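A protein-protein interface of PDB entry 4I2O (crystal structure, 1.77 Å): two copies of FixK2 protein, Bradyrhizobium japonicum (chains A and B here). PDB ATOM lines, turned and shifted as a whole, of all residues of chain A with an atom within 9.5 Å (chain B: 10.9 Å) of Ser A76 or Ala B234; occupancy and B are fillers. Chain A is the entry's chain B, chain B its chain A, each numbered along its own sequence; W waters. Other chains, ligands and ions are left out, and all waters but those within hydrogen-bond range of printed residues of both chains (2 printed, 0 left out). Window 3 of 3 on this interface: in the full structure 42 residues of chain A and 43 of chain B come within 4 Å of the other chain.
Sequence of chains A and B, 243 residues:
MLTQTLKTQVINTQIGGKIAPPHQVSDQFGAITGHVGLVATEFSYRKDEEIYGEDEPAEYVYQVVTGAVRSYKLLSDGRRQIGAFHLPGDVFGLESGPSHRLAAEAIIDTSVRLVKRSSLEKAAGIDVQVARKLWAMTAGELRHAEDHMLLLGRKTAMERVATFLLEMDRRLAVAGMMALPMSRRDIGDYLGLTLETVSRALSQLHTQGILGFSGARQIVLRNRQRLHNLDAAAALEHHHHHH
Water W2 lies within hydrogen-bond range of the side-chain carboxylate of Glu B159 and the guanidinium group of Arg A79.
Water W1 lies within hydrogen-bond range of N of Arg A80 and NE of Arg B154.
Printed residues of chain A that touch a printed residue of chain B: Lys A73, Leu A74, Leu A75, Ser A76, Arg A79 and Arg A80.
Among the printed residues, Asp or Glu carboxylates within 4 Å of a Lys or Arg side-chain nitrogen of the other chain: Lys A73 with Asp B147 and Arg A79 with Glu B159.
No position is printed for both chains.
The side-chain carboxylate of Glu A54 is in salt-bridge range of the side-chain amino group of Lys A73, 2.7 Å away.
NE of Arg A79 is in salt-bridge range of OD2 of Asp A77, 2.9 Å away.
OG1 of Thr B163 lies within hydrogen-bond range of O of Glu B159 (2.7 Å).
NZ of Lys B155 is in hydrogen-bond range of OG1 of Thr B163 (2.8 Å).
NZ of Lys A73 sits at hydrogen-bond distance from O of Arg A101.
Of the printed residues of chain B, Ser A76 touches Ala B233 (2.6 Å), Ala B234 (3.7 Å) and Ala B235 (3.7 Å).
Ala B234 touches two residues of chain A.
Of chain B, only Leu B150 (3.6 Å), Ala B232 (3.7 Å), Ala B233 (3.3 Å) and Ala B235 (3.9 Å) come within 4 Å of Leu A75.
Asp A77 touches none of the printed residues of chain B.
No residue of chain B comes within 4 Å of Gly A78.
Of chain A, only Leu A75 and Ser A76 come within 4 Å of Ala B233.
Ala B235 touches just these residues of chain A: Leu A74, Leu A75 and Ser A76.
Printed residues of chain A within 4 Å of Leu B150: Lys A73 and Leu A75.
Of the printed residues of chain B, Lys A73 touches Asp B147 and Leu B150.
Asp B231 touches none of the printed residues of chain A.
Leu B230 touches none of the printed residues of chain A.
The nearest residue of chain B that does not touch Ser A76 is Ala B232 (5.3 Å).
Leu B150 touches Lys A73.
Ala B234 touches Leu A74 (CA to O, 3.9 Å).
N of Ala B235 touches O of Leu A74, 3.5 Å away.
Leu A75 touches Leu B150.
Leu A75 touches Ala B233 (CA to O, 3.3 Å).
Ala B235 touches Leu A75.
CB of Ser A76 touches O of Ala B234 (3.7 Å).
Ser A76 touches Ala B235.
Lys B155 touches Arg A79 (CA to NH1, 3.9 Å).
Arg A79 touches Ala B232 (NH2 to CB, 3.6 Å).
O of Ala B233 is in hydrogen-bond range of N of Ser A76.
OE1 of Glu B159 is in salt-bridge range of NH1 of Arg A79 (2.8 Å).
The guanidinium group (NH1) of Arg A79 lies within hydrogen-bond range of the backbone carbonyl oxygen (O) of Arg B154, at 2.9 Å.
The guanidinium group (NE) of Arg B154 sits at hydrogen-bond distance from the backbone carbonyl oxygen (O) of Arg A80, at 2.9 Å.
The side-chain amino group (NZ) of Lys A73 is in salt-bridge range of the side-chain carboxylate (OD1) of Asp B147 (3.4 Å).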
ATOM      1  N   GLU A  54      16.787  -7.251  -4.849  1.00  0.00           N
ATOM      2  CA  GLU A  54      15.919  -6.177  -4.370  1.00  0.00           C
ATOM      3  C   GLU A  54      14.478  -6.653  -4.334  1.00  0.00           C
ATOM      4  O   GLU A  54      14.019  -7.311  -5.273  1.00  0.00           O
ATOM      5  CB  GLU A  54      16.056  -4.956  -5.276  1.00  0.00           C
ATOM      6  CG  GLU A  54      15.202  -3.773  -4.830  1.00  0.00           C
ATOM      7  CD  GLU A  54      15.628  -2.476  -5.498  1.00  0.00           C
ATOM      8  OE1 GLU A  54      16.591  -2.512  -6.308  1.00  0.00           O
ATOM      9  OE2 GLU A  54      15.004  -1.428  -5.200  1.00  0.00           O
ATOM     10  N   ASP A  55      13.775  -6.318  -3.247  1.00  0.00           N
ATOM     11  CA  ASP A  55      12.407  -6.765  -2.983  1.00  0.00           C
ATOM     12  C   ASP A  55      12.226  -8.235  -2.663  1.00  0.00           C
ATOM     13  O   ASP A  55      11.086  -8.676  -2.495  1.00  0.00           O
ATOM     14  CB  ASP A  55      11.446  -6.407  -4.128  1.00  0.00           C
ATOM     15  CG  ASP A  55      11.375  -4.925  -4.383  1.00  0.00           C
ATOM     16  OD1 ASP A  55      11.236  -4.139  -3.405  1.00  0.00           O
ATOM     17  OD2 ASP A  55      11.482  -4.559  -5.577  1.00  0.00           O
ATOM     18  N   LYS A  73      21.073  -0.371  -5.758  1.00  0.00           N
ATOM     19  CA  LYS A  73      19.795  -0.319  -6.416  1.00  0.00           C
ATOM     20  C   LYS A  73      20.029  -0.011  -7.888  1.00  0.00           C
ATOM     21  O   LYS A  73      20.981   0.692  -8.223  1.00  0.00           O
ATOM     22  CB  LYS A  73      18.972   0.856  -5.815  1.00  0.00           C
ATOM     23  CG  LYS A  73      18.511   0.662  -4.329  1.00  0.00           C
ATOM     24  CD  LYS A  73      17.626   1.832  -3.837  1.00  0.00           C
ATOM     25  CE  LYS A  73      16.635   1.375  -2.768  1.00  0.00           C
ATOM     26  NZ  LYS A  73      15.583   0.462  -3.366  1.00  0.00           N
ATOM     27  N   LEU A  74      19.141  -0.474  -8.758  1.00  0.00           N
ATOM     28  CA  LEU A  74      19.310  -0.224 -10.198  1.00  0.00           C
ATOM     29  C   LEU A  74      18.160   0.508 -10.764  1.00  0.00           C
ATOM     30  O   LEU A  74      17.056   0.369 -10.274  1.00  0.00           O
ATOM     31  CB  LEU A  74      19.297  -1.567 -10.947  1.00  0.00           C
ATOM     32  CG  LEU A  74      20.417  -2.536 -10.764  1.00  0.00           C
ATOM     33  CD1 LEU A  74      20.108  -3.804 -11.601  1.00  0.00           C
ATOM     34  CD2 LEU A  74      21.678  -1.877 -11.250  1.00  0.00           C
ATOM     35  N   LEU A  75      18.390   1.262 -11.838  1.00  0.00           N
ATOM     36  CA  LEU A  75      17.290   1.708 -12.632  1.00  0.00           C
ATOM     37  C   LEU A  75      17.185   0.859 -13.873  1.00  0.00           C
ATOM     38  O   LEU A  75      18.122   0.172 -14.281  1.00  0.00           O
ATOM     39  CB  LEU A  75      17.384   3.201 -12.989  1.00  0.00           C
ATOM     40  CG  LEU A  75      17.582   4.063 -11.754  1.00  0.00           C
ATOM     41  CD1 LEU A  75      17.988   5.430 -12.206  1.00  0.00           C
ATOM     42  CD2 LEU A  75      16.244   4.112 -10.972  1.00  0.00           C
ATOM     43  N   SER A  76      16.025   0.921 -14.494  1.00  0.00           N
ATOM     44  CA  SER A  76      15.763   0.041 -15.642  1.00  0.00           C
ATOM     45  C   SER A  76      16.730   0.167 -16.831  1.00  0.00           C
ATOM     46  O   SER A  76      16.945  -0.825 -17.570  1.00  0.00           O
ATOM     47  CB  SER A  76      14.364   0.302 -16.136  1.00  0.00           C
ATOM     48  OG  SER A  76      14.311   1.638 -16.568  1.00  0.00           O
ATOM     49  N   ASP A  77      17.321   1.351 -17.035  1.00  0.00           N
ATOM     50  CA  ASP A  77      18.273   1.457 -18.146  1.00  0.00           C
ATOM     51  C   ASP A  77      19.644   1.000 -17.734  1.00  0.00           C
ATOM     52  O   ASP A  77      20.577   1.102 -18.531  1.00  0.00           O
ATOM     53  CB  ASP A  77      18.347   2.862 -18.754  1.00  0.00           C
ATOM     54  CG  ASP A  77      18.846   3.893 -17.760  1.00  0.00           C
ATOM     55  OD1 ASP A  77      18.909   5.074 -18.141  1.00  0.00           O
ATOM     56  OD2 ASP A  77      19.133   3.557 -16.599  1.00  0.00           O
ATOM     57  N   GLY A  78      19.792   0.510 -16.498  1.00  0.00           N
ATOM     58  CA  GLY A  78      21.066  -0.059 -16.097  1.00  0.00           C
ATOM     59  C   GLY A  78      21.907   0.819 -15.208  1.00  0.00           C
ATOM     60  O   GLY A  78      22.998   0.424 -14.718  1.00  0.00           O
ATOM     61  N   ARG A  79      21.442   2.053 -14.971  1.00  0.00           N
ATOM     62  CA  ARG A  79      22.166   2.890 -14.045  1.00  0.00           C
ATOM     63  C   ARG A  79      22.110   2.279 -12.665  1.00  0.00           C
ATOM     64  O   ARG A  79      21.080   1.743 -12.282  1.00  0.00           O
ATOM     65  CB  ARG A  79      21.483   4.285 -13.998  1.00  0.00           C
ATOM     66  CG  ARG A  79      21.899   5.164 -15.227  1.00  0.00           C
ATOM     67  CD  ARG A  79      21.026   6.488 -15.016  1.00  0.00           C
ATOM     68  NE  ARG A  79      19.642   6.233 -15.487  1.00  0.00           N
ATOM     69  CZ  ARG A  79      18.651   7.120 -15.367  1.00  0.00           C
ATOM     70  NH1 ARG A  79      18.897   8.287 -14.806  1.00  0.00           N
ATOM     71  NH2 ARG A  79      17.424   6.862 -15.821  1.00  0.00           N
ATOM     72  N   ARG A  80      23.215   2.367 -11.920  1.00  0.00           N
ATOM     73  CA  ARG A  80      23.296   1.641 -10.648  1.00  0.00           C
ATOM     74  C   ARG A  80      23.899   2.547  -9.588  1.00  0.00           C
ATOM     75  O   ARG A  80      24.872   3.222  -9.887  1.00  0.00           O
ATOM     76  CB  ARG A  80      24.272   0.455 -10.844  1.00  0.00           C
ATOM     77  CG  ARG A  80      24.489  -0.267  -9.520  1.00  0.00           C
ATOM     78  CD  ARG A  80      25.444  -1.509  -9.781  1.00  0.00           C
ATOM     79  NE  ARG A  80      26.776  -1.045 -10.089  1.00  0.00           N
ATOM     80  CZ  ARG A  80      27.860  -1.815 -10.081  1.00  0.00           C
ATOM     81  NH1 ARG A  80      27.775  -3.086  -9.649  1.00  0.00           N
ATOM     82  NH2 ARG A  80      29.032  -1.276 -10.450  1.00  0.00           N
ATOM     83  N   ARG A 101      15.757  -4.194   0.621  1.00  0.00           N
ATOM     84  CA  ARG A 101      15.478  -2.956  -0.139  1.00  0.00           C
ATOM     85  C   ARG A 101      16.582  -2.662  -1.154  1.00  0.00           C
ATOM     86  O   ARG A 101      16.423  -1.761  -1.987  1.00  0.00           O
ATOM     87  CB  ARG A 101      15.317  -1.748   0.793  1.00  0.00           C
ATOM     88  CG  ARG A 101      14.289  -1.905   1.882  1.00  0.00           C
ATOM     89  CD  ARG A 101      12.905  -1.872   1.320  1.00  0.00           C
ATOM     90  NE  ARG A 101      11.951  -1.585   2.386  1.00  0.00           N
ATOM     91  CZ  ARG A 101      10.656  -1.872   2.325  1.00  0.00           C
ATOM     92  NH1 ARG A 101      10.160  -2.465   1.248  1.00  0.00           N
ATOM     93  NH2 ARG A 101       9.860  -1.570   3.347  1.00  0.00           N
ATOM     94  N   ASP B 147      16.517   5.152  -1.075  1.00  0.00           N
ATOM     95  CA  ASP B 147      15.904   5.613  -2.325  1.00  0.00           C
ATOM     96  C   ASP B 147      16.492   6.944  -2.699  1.00  0.00           C
ATOM     97  O   ASP B 147      16.722   7.219  -3.914  1.00  0.00           O
ATOM     98  CB  ASP B 147      14.366   5.790  -2.141  1.00  0.00           C
ATOM     99  CG  ASP B 147      13.616   4.468  -2.072  1.00  0.00           C
ATOM    100  OD1 ASP B 147      14.185   3.410  -2.438  1.00  0.00           O
ATOM    101  OD2 ASP B 147      12.421   4.492  -1.670  1.00  0.00           O
ATOM    102  N   LEU B 150      19.859   6.824  -4.454  1.00  0.00           N
ATOM    103  CA  LEU B 150      19.710   6.494  -5.866  1.00  0.00           C
ATOM    104  C   LEU B 150      19.365   7.746  -6.641  1.00  0.00           C
ATOM    105  O   LEU B 150      19.863   7.981  -7.732  1.00  0.00           O
ATOM    106  CB  LEU B 150      18.638   5.432  -6.069  1.00  0.00           C
ATOM    107  CG  LEU B 150      18.290   4.987  -7.495  1.00  0.00           C
ATOM    108  CD1 LEU B 150      19.518   4.426  -8.242  1.00  0.00           C
ATOM    109  CD2 LEU B 150      17.150   3.976  -7.520  1.00  0.00           C
ATOM    110  N   ARG B 154      22.110   9.068  -9.258  1.00  0.00           N
ATOM    111  CA  ARG B 154      21.897   8.548 -10.599  1.00  0.00           C
ATOM    112  C   ARG B 154      20.766   9.198 -11.439  1.00  0.00           C
ATOM    113  O   ARG B 154      20.768   9.012 -12.682  1.00  0.00           O
ATOM    114  CB  ARG B 154      21.719   6.998 -10.564  1.00  0.00           C
ATOM    115  CG  ARG B 154      22.986   6.305 -10.061  1.00  0.00           C
ATOM    116  CD  ARG B 154      23.946   6.320 -11.251  1.00  0.00           C
ATOM    117  NE  ARG B 154      25.350   5.852 -11.052  1.00  0.00           N
ATOM    118  CZ  ARG B 154      26.418   6.647 -11.200  1.00  0.00           C
ATOM    119  NH1 ARG B 154      26.259   7.957 -11.383  1.00  0.00           N
ATOM    120  NH2 ARG B 154      27.654   6.129 -11.203  1.00  0.00           N
ATOM    121  N   LYS B 155      19.825   9.973 -10.826  1.00  0.00           N
ATOM    122  CA  LYS B 155      18.668  10.446 -11.605  1.00  0.00           C
ATOM    123  C   LYS B 155      18.983  11.775 -12.313  1.00  0.00           C
ATOM    124  O   LYS B 155      19.828  12.552 -11.850  1.00  0.00           O
ATOM    125  CB  LYS B 155      17.362  10.614 -10.729  1.00  0.00           C
ATOM    126  CG  LYS B 155      16.747   9.245 -10.429  1.00  0.00           C
ATOM    127  CD  LYS B 155      15.403   9.432  -9.659  1.00  0.00           C
ATOM    128  CE  LYS B 155      14.771   8.047  -9.374  1.00  0.00           C
ATOM    129  NZ  LYS B 155      13.359   8.250  -8.768  1.00  0.00           N
ATOM    130  N   GLU B 159      14.068  13.733 -13.801  1.00  0.00           N
ATOM    131  CA  GLU B 159      13.657  12.597 -12.938  1.00  0.00           C
ATOM    132  C   GLU B 159      13.583  12.915 -11.481  1.00  0.00           C
ATOM    133  O   GLU B 159      12.695  12.386 -10.741  1.00  0.00           O
ATOM    134  CB  GLU B 159      14.651  11.408 -13.197  1.00  0.00           C
ATOM    135  CG  GLU B 159      14.533  10.808 -14.578  1.00  0.00           C
ATOM    136  CD  GLU B 159      15.724   9.879 -14.892  1.00  0.00           C
ATOM    137  OE1 GLU B 159      16.778   9.972 -14.171  1.00  0.00           O
ATOM    138  OE2 GLU B 159      15.683   9.188 -15.943  1.00  0.00           O
ATOM    139  N   THR B 163      10.170  12.877  -9.373  1.00  0.00           N
ATOM    140  CA  THR B 163      10.094  12.048  -8.132  1.00  0.00           C
ATOM    141  C   THR B 163       9.562  12.904  -6.981  1.00  0.00           C
ATOM    142  O   THR B 163       8.662  12.487  -6.252  1.00  0.00           O
ATOM    143  CB  THR B 163      11.466  11.485  -7.744  1.00  0.00           C
ATOM    144  OG1 THR B 163      11.864  10.667  -8.818  1.00  0.00           O
ATOM    145  CG2 THR B 163      11.341  10.582  -6.459  1.00  0.00           C
ATOM    146  N   HIS B 228       4.906  10.139 -13.680  1.00  0.00           N
ATOM    147  CA  HIS B 228       5.562   8.897 -13.269  1.00  0.00           C
ATOM    148  C   HIS B 228       6.463   8.438 -14.414  1.00  0.00           C
ATOM    149  O   HIS B 228       7.549   7.894 -14.176  1.00  0.00           O
ATOM    150  CB  HIS B 228       4.536   7.780 -13.107  1.00  0.00           C
ATOM    151  CG  HIS B 228       4.486   7.179 -11.746  1.00  0.00           C
ATOM    152  ND1 HIS B 228       5.445   6.304 -11.283  1.00  0.00           N
ATOM    153  CD2 HIS B 228       3.566   7.304 -10.750  1.00  0.00           C
ATOM    154  CE1 HIS B 228       5.126   5.928 -10.053  1.00  0.00           C
ATOM    155  NE2 HIS B 228       3.995   6.524  -9.705  1.00  0.00           N
ATOM    156  N   ASN B 229       6.026   8.613 -15.658  1.00  0.00           N
ATOM    157  CA  ASN B 229       6.902   8.190 -16.790  1.00  0.00           C
ATOM    158  C   ASN B 229       8.200   8.966 -16.945  1.00  0.00           C
ATOM    159  O   ASN B 229       9.064   8.560 -17.750  1.00  0.00           O
ATOM    160  CB  ASN B 229       6.192   8.280 -18.135  1.00  0.00           C
ATOM    161  CG  ASN B 229       5.013   7.376 -18.215  1.00  0.00           C
ATOM    162  OD1 ASN B 229       4.877   6.442 -17.418  1.00  0.00           O
ATOM    163  ND2 ASN B 229       4.104   7.677 -19.138  1.00  0.00           N
ATOM    164  N   LEU B 230       8.286  10.112 -16.279  1.00  0.00           N
ATOM    165  CA  LEU B 230       9.476  10.948 -16.337  1.00  0.00           C
ATOM    166  C   LEU B 230      10.386  10.674 -15.161  1.00  0.00           C
ATOM    167  O   LEU B 230      11.485  11.225 -15.098  1.00  0.00           O
ATOM    168  CB  LEU B 230       9.090  12.426 -16.306  1.00  0.00           C
ATOM    169  CG  LEU B 230       8.302  12.926 -17.528  1.00  0.00           C
ATOM    170  CD1 LEU B 230       8.029  14.395 -17.334  1.00  0.00           C
ATOM    171  CD2 LEU B 230       9.104  12.719 -18.816  1.00  0.00           C
ATOM    172  N   ASP B 231       9.941   9.880 -14.188  1.00  0.00           N
ATOM    173  CA  ASP B 231      10.867   9.536 -13.168  1.00  0.00           C
ATOM    174  C   ASP B 231      11.640   8.327 -13.798  1.00  0.00           C
ATOM    175  O   ASP B 231      11.429   7.957 -14.963  1.00  0.00           O
ATOM    176  CB  ASP B 231      10.235   9.357 -11.770  1.00  0.00           C
ATOM    177  CG  ASP B 231       9.355   8.117 -11.615  1.00  0.00           C
ATOM    178  OD1 ASP B 231       9.543   7.092 -12.325  1.00  0.00           O
ATOM    179  OD2 ASP B 231       8.477   8.164 -10.705  1.00  0.00           O
ATOM    180  N   ALA B 232      12.551   7.736 -13.087  1.00  0.00           N
ATOM    181  CA  ALA B 232      13.254   6.621 -13.737  1.00  0.00           C
ATOM    182  C   ALA B 232      12.658   5.357 -13.131  1.00  0.00           C
ATOM    183  O   ALA B 232      12.281   5.375 -11.965  1.00  0.00           O
ATOM    184  CB  ALA B 232      14.722   6.723 -13.446  1.00  0.00           C
ATOM    185  N   ALA B 233      12.563   4.261 -13.879  1.00  0.00           N
ATOM    186  CA  ALA B 233      11.921   3.065 -13.296  1.00  0.00           C
ATOM    187  C   ALA B 233      12.924   2.063 -12.774  1.00  0.00           C
ATOM    188  O   ALA B 233      14.058   2.017 -13.248  1.00  0.00           O
ATOM    189  CB  ALA B 233      10.973   2.392 -14.275  1.00  0.00           C
ATOM    190  N   ALA B 234      12.488   1.263 -11.799  1.00  0.00           N
ATOM    191  CA  ALA B 234      13.312   0.233 -11.198  1.00  0.00           C
ATOM    192  C   ALA B 234      13.551  -0.865 -12.216  1.00  0.00           C
ATOM    193  O   ALA B 234      12.722  -1.071 -13.116  1.00  0.00           O
ATOM    194  CB  ALA B 234      12.632  -0.337  -9.951  1.00  0.00           C
ATOM    195  N   ALA B 235      14.684  -1.556 -12.060  1.00  0.00           N
ATOM    196  CA  ALA B 235      15.080  -2.650 -12.930  1.00  0.00           C
ATOM    197  C   ALA B 235      14.133  -3.844 -12.798  1.00  0.00           C
ATOM    198  O   ALA B 235      13.650  -4.145 -11.708  1.00  0.00           O
ATOM    199  CB  ALA B 235      16.494  -3.067 -12.607  1.00  0.00           C
HETATM  200  O   HOH W   1      25.623   3.426 -13.221  1.00  0.00           O
HETATM  201  O   HOH W   2      17.364   9.319 -18.177  1.00  0.00           O
